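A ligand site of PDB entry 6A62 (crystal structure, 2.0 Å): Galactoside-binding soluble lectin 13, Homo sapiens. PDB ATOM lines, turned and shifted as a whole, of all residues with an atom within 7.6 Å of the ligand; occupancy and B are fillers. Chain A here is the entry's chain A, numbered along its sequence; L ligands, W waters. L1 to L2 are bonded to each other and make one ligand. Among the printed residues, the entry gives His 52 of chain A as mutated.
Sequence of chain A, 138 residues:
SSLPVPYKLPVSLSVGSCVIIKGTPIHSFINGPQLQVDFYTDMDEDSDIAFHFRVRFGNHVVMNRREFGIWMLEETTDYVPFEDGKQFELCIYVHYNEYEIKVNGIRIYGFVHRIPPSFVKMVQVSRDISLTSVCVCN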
ATOM      1  N   GLN A  34      15.310 -11.140  25.354  1.00  0.00           N
ATOM      2  CA  GLN A  34      15.184  -9.781  24.828  1.00  0.00           C
ATOM      3  C   GLN A  34      13.737  -9.340  24.864  1.00  0.00           C
ATOM      4  O   GLN A  34      12.816 -10.164  24.879  1.00  0.00           O
ATOM      5  CB  GLN A  34      15.716  -9.672  23.388  1.00  0.00           C
ATOM      6  CG  GLN A  34      17.229  -9.862  23.277  1.00  0.00           C
ATOM      7  CD  GLN A  34      17.732  -9.978  21.849  1.00  0.00           C
ATOM      8  OE1 GLN A  34      18.842 -10.441  21.610  1.00  0.00           O
ATOM      9  NE2 GLN A  34      16.909  -9.576  20.894  1.00  0.00           N
ATOM     10  N   GLN A  36      11.416  -6.234  22.775  1.00  0.00           N
ATOM     11  CA  GLN A  36      11.468  -5.235  21.709  1.00  0.00           C
ATOM     12  C   GLN A  36      10.148  -4.465  21.628  1.00  0.00           C
ATOM     13  O   GLN A  36       9.072  -5.079  21.621  1.00  0.00           O
ATOM     14  CB  GLN A  36      11.774  -5.869  20.348  1.00  0.00           C
ATOM     15  CG  GLN A  36      12.112  -4.820  19.282  1.00  0.00           C
ATOM     16  CD  GLN A  36      12.669  -5.410  18.005  1.00  0.00           C
ATOM     17  OE1 GLN A  36      13.623  -6.188  18.009  1.00  0.00           O
ATOM     18  NE2 GLN A  36      12.021  -5.058  16.883  1.00  0.00           N
ATOM     19  N   ASP A  38       8.495  -1.448  19.096  1.00  0.00           N
ATOM     20  CA  ASP A  38       8.632  -0.634  17.891  1.00  0.00           C
ATOM     21  C   ASP A  38       7.439   0.308  17.780  1.00  0.00           C
ATOM     22  O   ASP A  38       6.294  -0.133  17.888  1.00  0.00           O
ATOM     23  CB  ASP A  38       8.722  -1.479  16.627  1.00  0.00           C
ATOM     24  CG  ASP A  38       9.973  -2.337  16.577  1.00  0.00           C
ATOM     25  OD1 ASP A  38      11.084  -1.787  16.371  1.00  0.00           O
ATOM     26  OD2 ASP A  38       9.849  -3.576  16.729  1.00  0.00           O
ATOM     27  N   ILE A  49       9.889   3.220  11.116  1.00  0.00           N
ATOM     28  CA  ILE A  49       9.781   3.080  12.563  1.00  0.00           C
ATOM     29  C   ILE A  49      10.289   4.364  13.197  1.00  0.00           C
ATOM     30  O   ILE A  49      11.461   4.714  13.037  1.00  0.00           O
ATOM     31  CB  ILE A  49      10.586   1.873  13.071  1.00  0.00           C
ATOM     32  CG1 ILE A  49      10.011   0.574  12.483  1.00  0.00           C
ATOM     33  CG2 ILE A  49      10.604   1.808  14.610  1.00  0.00           C
ATOM     34  CD1 ILE A  49      10.910  -0.642  12.736  1.00  0.00           C
ATOM     35  N   HIS A  52      12.543   2.587  17.836  1.00  0.00           N
ATOM     36  CA  HIS A  52      12.812   1.166  18.014  1.00  0.00           C
ATOM     37  C   HIS A  52      13.613   1.014  19.299  1.00  0.00           C
ATOM     38  O   HIS A  52      14.620   1.713  19.494  1.00  0.00           O
ATOM     39  CB  HIS A  52      13.581   0.629  16.798  1.00  0.00           C
ATOM     40  CG  HIS A  52      14.306  -0.664  17.045  1.00  0.00           C
ATOM     41  ND1 HIS A  52      13.685  -1.894  16.975  1.00  0.00           N
ATOM     42  CD2 HIS A  52      15.609  -0.912  17.288  1.00  0.00           C
ATOM     43  CE1 HIS A  52      14.571  -2.846  17.203  1.00  0.00           C
ATOM     44  NE2 HIS A  52      15.749  -2.279  17.386  1.00  0.00           N
ATOM     45  N   PHE A  53      13.157   0.139  20.173  1.00  0.00           N
ATOM     46  CA  PHE A  53      13.716  -0.030  21.516  1.00  0.00           C
ATOM     47  C   PHE A  53      13.901  -1.519  21.749  1.00  0.00           C
ATOM     48  O   PHE A  53      12.934  -2.279  21.715  1.00  0.00           O
ATOM     49  CB  PHE A  53      12.758   0.596  22.531  1.00  0.00           C
ATOM     50  CG  PHE A  53      13.115   0.355  23.972  1.00  0.00           C
ATOM     51  CD1 PHE A  53      13.984   1.198  24.643  1.00  0.00           C
ATOM     52  CD2 PHE A  53      12.492  -0.661  24.692  1.00  0.00           C
ATOM     53  CE1 PHE A  53      14.279   1.000  25.975  1.00  0.00           C
ATOM     54  CE2 PHE A  53      12.778  -0.863  26.024  1.00  0.00           C
ATOM     55  CZ  PHE A  53      13.670  -0.028  26.671  1.00  0.00           C
ATOM     56  N   ARG A  54      15.142  -1.953  21.942  1.00  0.00           N
ATOM     57  CA  ARG A  54      15.432  -3.385  22.036  1.00  0.00           C
ATOM     58  C   ARG A  54      16.324  -3.651  23.248  1.00  0.00           C
ATOM     59  O   ARG A  54      17.502  -3.311  23.247  1.00  0.00           O
ATOM     60  CB  ARG A  54      16.105  -3.867  20.756  1.00  0.00           C
ATOM     61  CG  ARG A  54      16.346  -5.357  20.719  1.00  0.00           C
ATOM     62  CD  ARG A  54      16.482  -5.757  19.279  1.00  0.00           C
ATOM     63  NE  ARG A  54      17.112  -7.034  19.124  1.00  0.00           N
ATOM     64  CZ  ARG A  54      17.394  -7.585  17.945  1.00  0.00           C
ATOM     65  NH1 ARG A  54      17.095  -6.934  16.828  1.00  0.00           N
ATOM     66  NH2 ARG A  54      17.965  -8.790  17.884  1.00  0.00           N
ATOM     67  N   HIS A  60      22.345  -4.630  27.704  1.00  0.00           N
ATOM     68  CA  HIS A  60      22.257  -3.243  27.257  1.00  0.00           C
ATOM     69  C   HIS A  60      20.970  -3.052  26.471  1.00  0.00           C
ATOM     70  O   HIS A  60      20.219  -4.004  26.221  1.00  0.00           O
ATOM     71  CB  HIS A  60      23.486  -2.845  26.416  1.00  0.00           C
ATOM     72  CG  HIS A  60      23.561  -3.545  25.098  1.00  0.00           C
ATOM     73  ND1 HIS A  60      24.244  -4.727  24.914  1.00  0.00           N
ATOM     74  CD2 HIS A  60      23.027  -3.240  23.886  1.00  0.00           C
ATOM     75  CE1 HIS A  60      24.134  -5.110  23.658  1.00  0.00           C
ATOM     76  NE2 HIS A  60      23.400  -4.226  23.010  1.00  0.00           N
ATOM     77  N   VAL A  62      19.447  -1.216  22.902  1.00  0.00           N
ATOM     78  CA  VAL A  62      19.698  -0.591  21.605  1.00  0.00           C
ATOM     79  C   VAL A  62      18.454   0.165  21.169  1.00  0.00           C
ATOM     80  O   VAL A  62      17.332  -0.352  21.268  1.00  0.00           O
ATOM     81  CB  VAL A  62      20.110  -1.645  20.556  1.00  0.00           C
ATOM     82  CG1 VAL A  62      19.972  -1.080  19.158  1.00  0.00           C
ATOM     83  CG2 VAL A  62      21.535  -2.106  20.815  1.00  0.00           C
ATOM     84  N   MET A  63      18.646   1.394  20.694  1.00  0.00           N
ATOM     85  CA  MET A  63      17.548   2.235  20.208  1.00  0.00           C
ATOM     86  C   MET A  63      17.901   2.794  18.841  1.00  0.00           C
ATOM     87  O   MET A  63      19.058   3.110  18.568  1.00  0.00           O
ATOM     88  CB  MET A  63      17.245   3.372  21.170  1.00  0.00           C
ATOM     89  CG  MET A  63      16.514   2.917  22.401  1.00  0.00           C
ATOM     90  SD  MET A  63      16.708   4.091  23.731  1.00  0.00           S
ATOM     91  CE  MET A  63      18.514   4.028  23.869  1.00  0.00           C
ATOM     92  N   ASN A  64      16.899   2.927  17.974  1.00  0.00           N
ATOM     93  CA  ASN A  64      17.141   3.443  16.637  1.00  0.00           C
ATOM     94  C   ASN A  64      15.815   3.869  16.019  1.00  0.00           C
ATOM     95  O   ASN A  64      14.743   3.762  16.635  1.00  0.00           O
ATOM     96  CB  ASN A  64      17.836   2.404  15.747  1.00  0.00           C
ATOM     97  CG  ASN A  64      18.715   3.015  14.655  1.00  0.00           C
ATOM     98  OD1 ASN A  64      18.661   4.214  14.379  1.00  0.00           O
ATOM     99  ND2 ASN A  64      19.553   2.189  14.031  1.00  0.00           N
ATOM    100  N   ARG A  65      15.902   4.333  14.787  1.00  0.00           N
ATOM    101  CA  ARG A  65      14.710   4.505  13.977  1.00  0.00           C
ATOM    102  C   ARG A  65      15.033   4.018  12.567  1.00  0.00           C
ATOM    103  O   ARG A  65      16.195   3.829  12.205  1.00  0.00           O
ATOM    104  CB  ARG A  65      14.245   5.975  13.989  1.00  0.00           C
ATOM    105  CG  ARG A  65      15.172   6.861  13.280  1.00  0.00           C
ATOM    106  CD  ARG A  65      15.740   7.959  14.153  1.00  0.00           C
ATOM    107  NE  ARG A  65      16.349   8.928  13.259  1.00  0.00           N
ATOM    108  CZ  ARG A  65      17.633   9.276  13.226  1.00  0.00           C
ATOM    109  NH1 ARG A  65      18.499   8.763  14.084  1.00  0.00           N
ATOM    110  NH2 ARG A  65      18.026  10.161  12.320  1.00  0.00           N
ATOM    111  N   ARG A  66      13.981   3.771  11.792  1.00  0.00           N
ATOM    112  CA  ARG A  66      14.115   3.316  10.418  1.00  0.00           C
ATOM    113  C   ARG A  66      13.381   4.303   9.517  1.00  0.00           C
ATOM    114  O   ARG A  66      12.160   4.458   9.629  1.00  0.00           O
ATOM    115  CB  ARG A  66      13.543   1.914  10.235  1.00  0.00           C
ATOM    116  CG  ARG A  66      13.916   1.283   8.907  1.00  0.00           C
ATOM    117  CD  ARG A  66      13.672  -0.223   8.928  1.00  0.00           C
ATOM    118  NE  ARG A  66      12.252  -0.547   8.909  1.00  0.00           N
ATOM    119  CZ  ARG A  66      11.749  -1.708   9.327  1.00  0.00           C
ATOM    120  NH1 ARG A  66      12.579  -2.636   9.817  1.00  0.00           N
ATOM    121  NH2 ARG A  66      10.447  -1.931   9.283  1.00  0.00           N
ATOM    122  N   TRP A  71      17.956   1.680   8.442  1.00  0.00           N
ATOM    123  CA  TRP A  71      18.248   1.957   9.848  1.00  0.00           C
ATOM    124  C   TRP A  71      19.216   3.137   9.962  1.00  0.00           C
ATOM    125  O   TRP A  71      20.155   3.264   9.181  1.00  0.00           O
ATOM    126  CB  TRP A  71      18.825   0.723  10.523  1.00  0.00           C
ATOM    127  CG  TRP A  71      17.816  -0.387  10.704  1.00  0.00           C
ATOM    128  CD1 TRP A  71      17.715  -1.540   9.972  1.00  0.00           C
ATOM    129  CD2 TRP A  71      16.791  -0.461  11.692  1.00  0.00           C
ATOM    130  NE1 TRP A  71      16.684  -2.314  10.440  1.00  0.00           N
ATOM    131  CE2 TRP A  71      16.102  -1.682  11.500  1.00  0.00           C
ATOM    132  CE3 TRP A  71      16.385   0.386  12.731  1.00  0.00           C
ATOM    133  CZ2 TRP A  71      15.031  -2.070  12.303  1.00  0.00           C
ATOM    134  CZ3 TRP A  71      15.312  -0.002  13.524  1.00  0.00           C
ATOM    135  CH2 TRP A  71      14.651  -1.217  13.309  1.00  0.00           C
ATOM    136  N   MET A  72      18.973   4.000  10.942  1.00  0.00           N
ATOM    137  CA  MET A  72      19.765   5.213  11.120  1.00  0.00           C
ATOM    138  C   MET A  72      20.849   4.980  12.171  1.00  0.00           C
ATOM    139  O   MET A  72      21.246   3.826  12.429  1.00  0.00           O
ATOM    140  CB  MET A  72      18.823   6.386  11.476  1.00  0.00           C
ATOM    141  CG  MET A  72      17.725   6.654  10.451  1.00  0.00           C
ATOM    142  SD  MET A  72      18.356   6.963   8.774  1.00  0.00           S
ATOM    143  CE  MET A  72      18.679   8.704   8.897  1.00  0.00           C
ATOM    144  N   LEU A  73      21.336   6.045  12.797  1.00  0.00           N
ATOM    145  CA  LEU A  73      22.440   5.915  13.733  1.00  0.00           C
ATOM    146  C   LEU A  73      21.953   5.304  15.041  1.00  0.00           C
ATOM    147  O   LEU A  73      21.102   5.882  15.734  1.00  0.00           O
ATOM    148  CB  LEU A  73      23.108   7.269  14.001  1.00  0.00           C
ATOM    149  CG  LEU A  73      24.512   7.079  14.611  1.00  0.00           C
ATOM    150  CD1 LEU A  73      25.363   6.139  13.752  1.00  0.00           C
ATOM    151  CD2 LEU A  73      25.236   8.393  14.797  1.00  0.00           C
ATOM    152  N   GLU A  74      22.516   4.165  15.402  1.00  0.00           N
ATOM    153  CA  GLU A  74      22.104   3.441  16.589  1.00  0.00           C
ATOM    154  C   GLU A  74      22.471   4.204  17.849  1.00  0.00           C
ATOM    155  O   GLU A  74      23.563   4.753  17.970  1.00  0.00           O
ATOM    156  CB  GLU A  74      22.783   2.085  16.592  1.00  0.00           C
ATOM    157  CG  GLU A  74      21.958   0.961  17.063  1.00  0.00           C
ATOM    158  CD  GLU A  74      22.646  -0.346  16.766  1.00  0.00           C
ATOM    159  OE1 GLU A  74      22.172  -1.078  15.866  1.00  0.00           O
ATOM    160  OE2 GLU A  74      23.691  -0.613  17.403  1.00  0.00           O
ATOM    161  N   GLU A  75      21.555   4.225  18.813  1.00  0.00           N
ATOM    162  CA  GLU A  75      21.802   4.758  20.148  1.00  0.00           C
ATOM    163  C   GLU A  75      21.739   3.629  21.163  1.00  0.00           C
ATOM    164  O   GLU A  75      21.057   2.626  20.940  1.00  0.00           O
ATOM    165  CB  GLU A  75      20.792   5.859  20.485  1.00  0.00           C
ATOM    166  CG  GLU A  75      20.753   6.961  19.419  1.00  0.00           C
ATOM    167  CD  GLU A  75      19.702   8.044  19.678  1.00  0.00           C
ATOM    168  OE1 GLU A  75      19.499   8.421  20.851  1.00  0.00           O
ATOM    169  OE2 GLU A  75      19.098   8.516  18.693  1.00  0.00           O
ATOM    170  N   ARG A 127       9.281 -10.373  21.112  1.00  0.00           N
ATOM    171  CA  ARG A 127      10.368 -11.238  21.587  1.00  0.00           C
ATOM    172  C   ARG A 127      10.040 -11.955  22.895  1.00  0.00           C
ATOM    173  O   ARG A 127       8.920 -12.440  23.078  1.00  0.00           O
ATOM    174  CB  ARG A 127      11.678 -10.451  21.652  1.00  0.00           C
ATOM    175  CG  ARG A 127      12.034  -9.953  20.259  1.00  0.00           C
ATOM    176  CD  ARG A 127      13.486  -9.639  20.071  1.00  0.00           C
ATOM    177  NE  ARG A 127      13.669  -8.908  18.822  1.00  0.00           N
ATOM    178  CZ  ARG A 127      14.153  -9.432  17.702  1.00  0.00           C
ATOM    179  NH1 ARG A 127      14.258  -8.672  16.617  1.00  0.00           N
ATOM    180  NH2 ARG A 127      14.539 -10.712  17.657  1.00  0.00           N
HETATM  181  C1  LIG L   1      24.485  -3.707  14.337  1.00  0.00           C
HETATM  182  C2  LIG L   1      23.219  -4.384  14.630  1.00  0.00           C
HETATM  183  C3  LIG L   1      22.261  -4.183  13.582  1.00  0.00           C
HETATM  184  C4  LIG L   1      22.804  -4.630  12.270  1.00  0.00           C
HETATM  185  C5  LIG L   1      21.794  -4.406  11.129  1.00  0.00           C
HETATM  186  C6  LIG L   1      25.095  -4.271  13.046  1.00  0.00           C
HETATM  187  O1  LIG L   1      26.214  -3.654  12.786  1.00  0.00           O
HETATM  188  O2  LIG L   1      25.409  -3.920  15.439  1.00  0.00           O
HETATM  189  O3  LIG L   1      22.682  -3.878  15.937  1.00  0.00           O
HETATM  190  O4  LIG L   1      21.070  -5.042  13.910  1.00  0.00           O
HETATM  191  O5  LIG L   1      24.079  -4.001  11.951  1.00  0.00           O
HETATM  192  O6  LIG L   1      21.895  -3.097  10.663  1.00  0.00           O
HETATM  193  C1  LG2 L   2      19.920  -4.359  13.659  1.00  0.00           C
HETATM  194  C2  LG2 L   2      18.744  -5.316  13.875  1.00  0.00           C
HETATM  195  C3  LG2 L   2      17.434  -4.600  13.889  1.00  0.00           C
HETATM  196  C4  LG2 L   2      17.433  -3.455  14.815  1.00  0.00           C
HETATM  197  C5  LG2 L   2      18.563  -2.491  14.484  1.00  0.00           C
HETATM  198  C6  LG2 L   2      18.577  -1.414  15.473  1.00  0.00           C
HETATM  199  O1  LG2 L   2      18.742  -6.258  12.836  1.00  0.00           O
HETATM  200  O2  LG2 L   2      16.391  -5.555  14.270  1.00  0.00           O
HETATM  201  O3  LG2 L   2      17.650  -3.934  16.170  1.00  0.00           O
HETATM  202  O4  LG2 L   2      19.894  -3.194  14.529  1.00  0.00           O
HETATM  203  O5  LG2 L   2      19.602  -0.554  15.155  1.00  0.00           O
HETATM  204  O   HOH W   1      21.312  -0.740  12.400  1.00  0.00           O
HETATM  205  O   HOH W   2      13.756  -5.139  14.762  1.00  0.00           O
HETATM  206  O   HOH W   3      20.213  -4.954  17.675  1.00  0.00           O
HETATM  207  O   HOH W   4      18.065  -5.567  10.524  1.00  0.00           O
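The backbone carbonyl oxygen (O) of Asn 64 lies within hydrogen-bond range of the backbone NH (N) of His 52 (2.8 Å). The side-chain carboxylate of Asp 38 sits at hydrogen-bond distance from a ring nitrogen (ND1) of His 52, 2.7 Å away. The side-chain amide nitrogen (ND2) of Asn 64 lies within hydrogen-bond range of the backbone carbonyl oxygen (O) of Met 72, 2.8 Å away. OD1 of Asn 64 lies close to O of Leu 73 (3.3 Å). The backbone NH (N) of Arg 54 is in hydrogen-bond range of the backbone carbonyl oxygen (O) of Val 62, at 2.8 Å. The guanidinium group (NE) of Arg 54 lies close to the side-chain amide nitrogen (NE2) of Gln 34, at 3.1 Å.
Merely in contact with the ligand: Val 62 and Trp 71. Hydrophobic or aromatic side chains within 4 Å of the ligand: His 52, Val 62 and Trp 71.
Water W2 lies within hydrogen-bond range of an oxygen (O2) of LG2 L2 and the side-chain amide nitrogen of Gln 36.
The side-chain carboxylate (OE1) of Glu 74 is in hydrogen-bond range of an oxygen (O5) of LG2 L2 (2.7 Å). O3 of LG2 L2 lies within hydrogen-bond range of NE2 of His 52 (2.8 Å). O5 of LG2 L2 is in hydrogen-bond range of ND2 of Asn 64. An oxygen (O2) of LG2 L2 lies within hydrogen-bond range of the guanidinium group (NH1) of Arg 54, 3.0 Å away.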
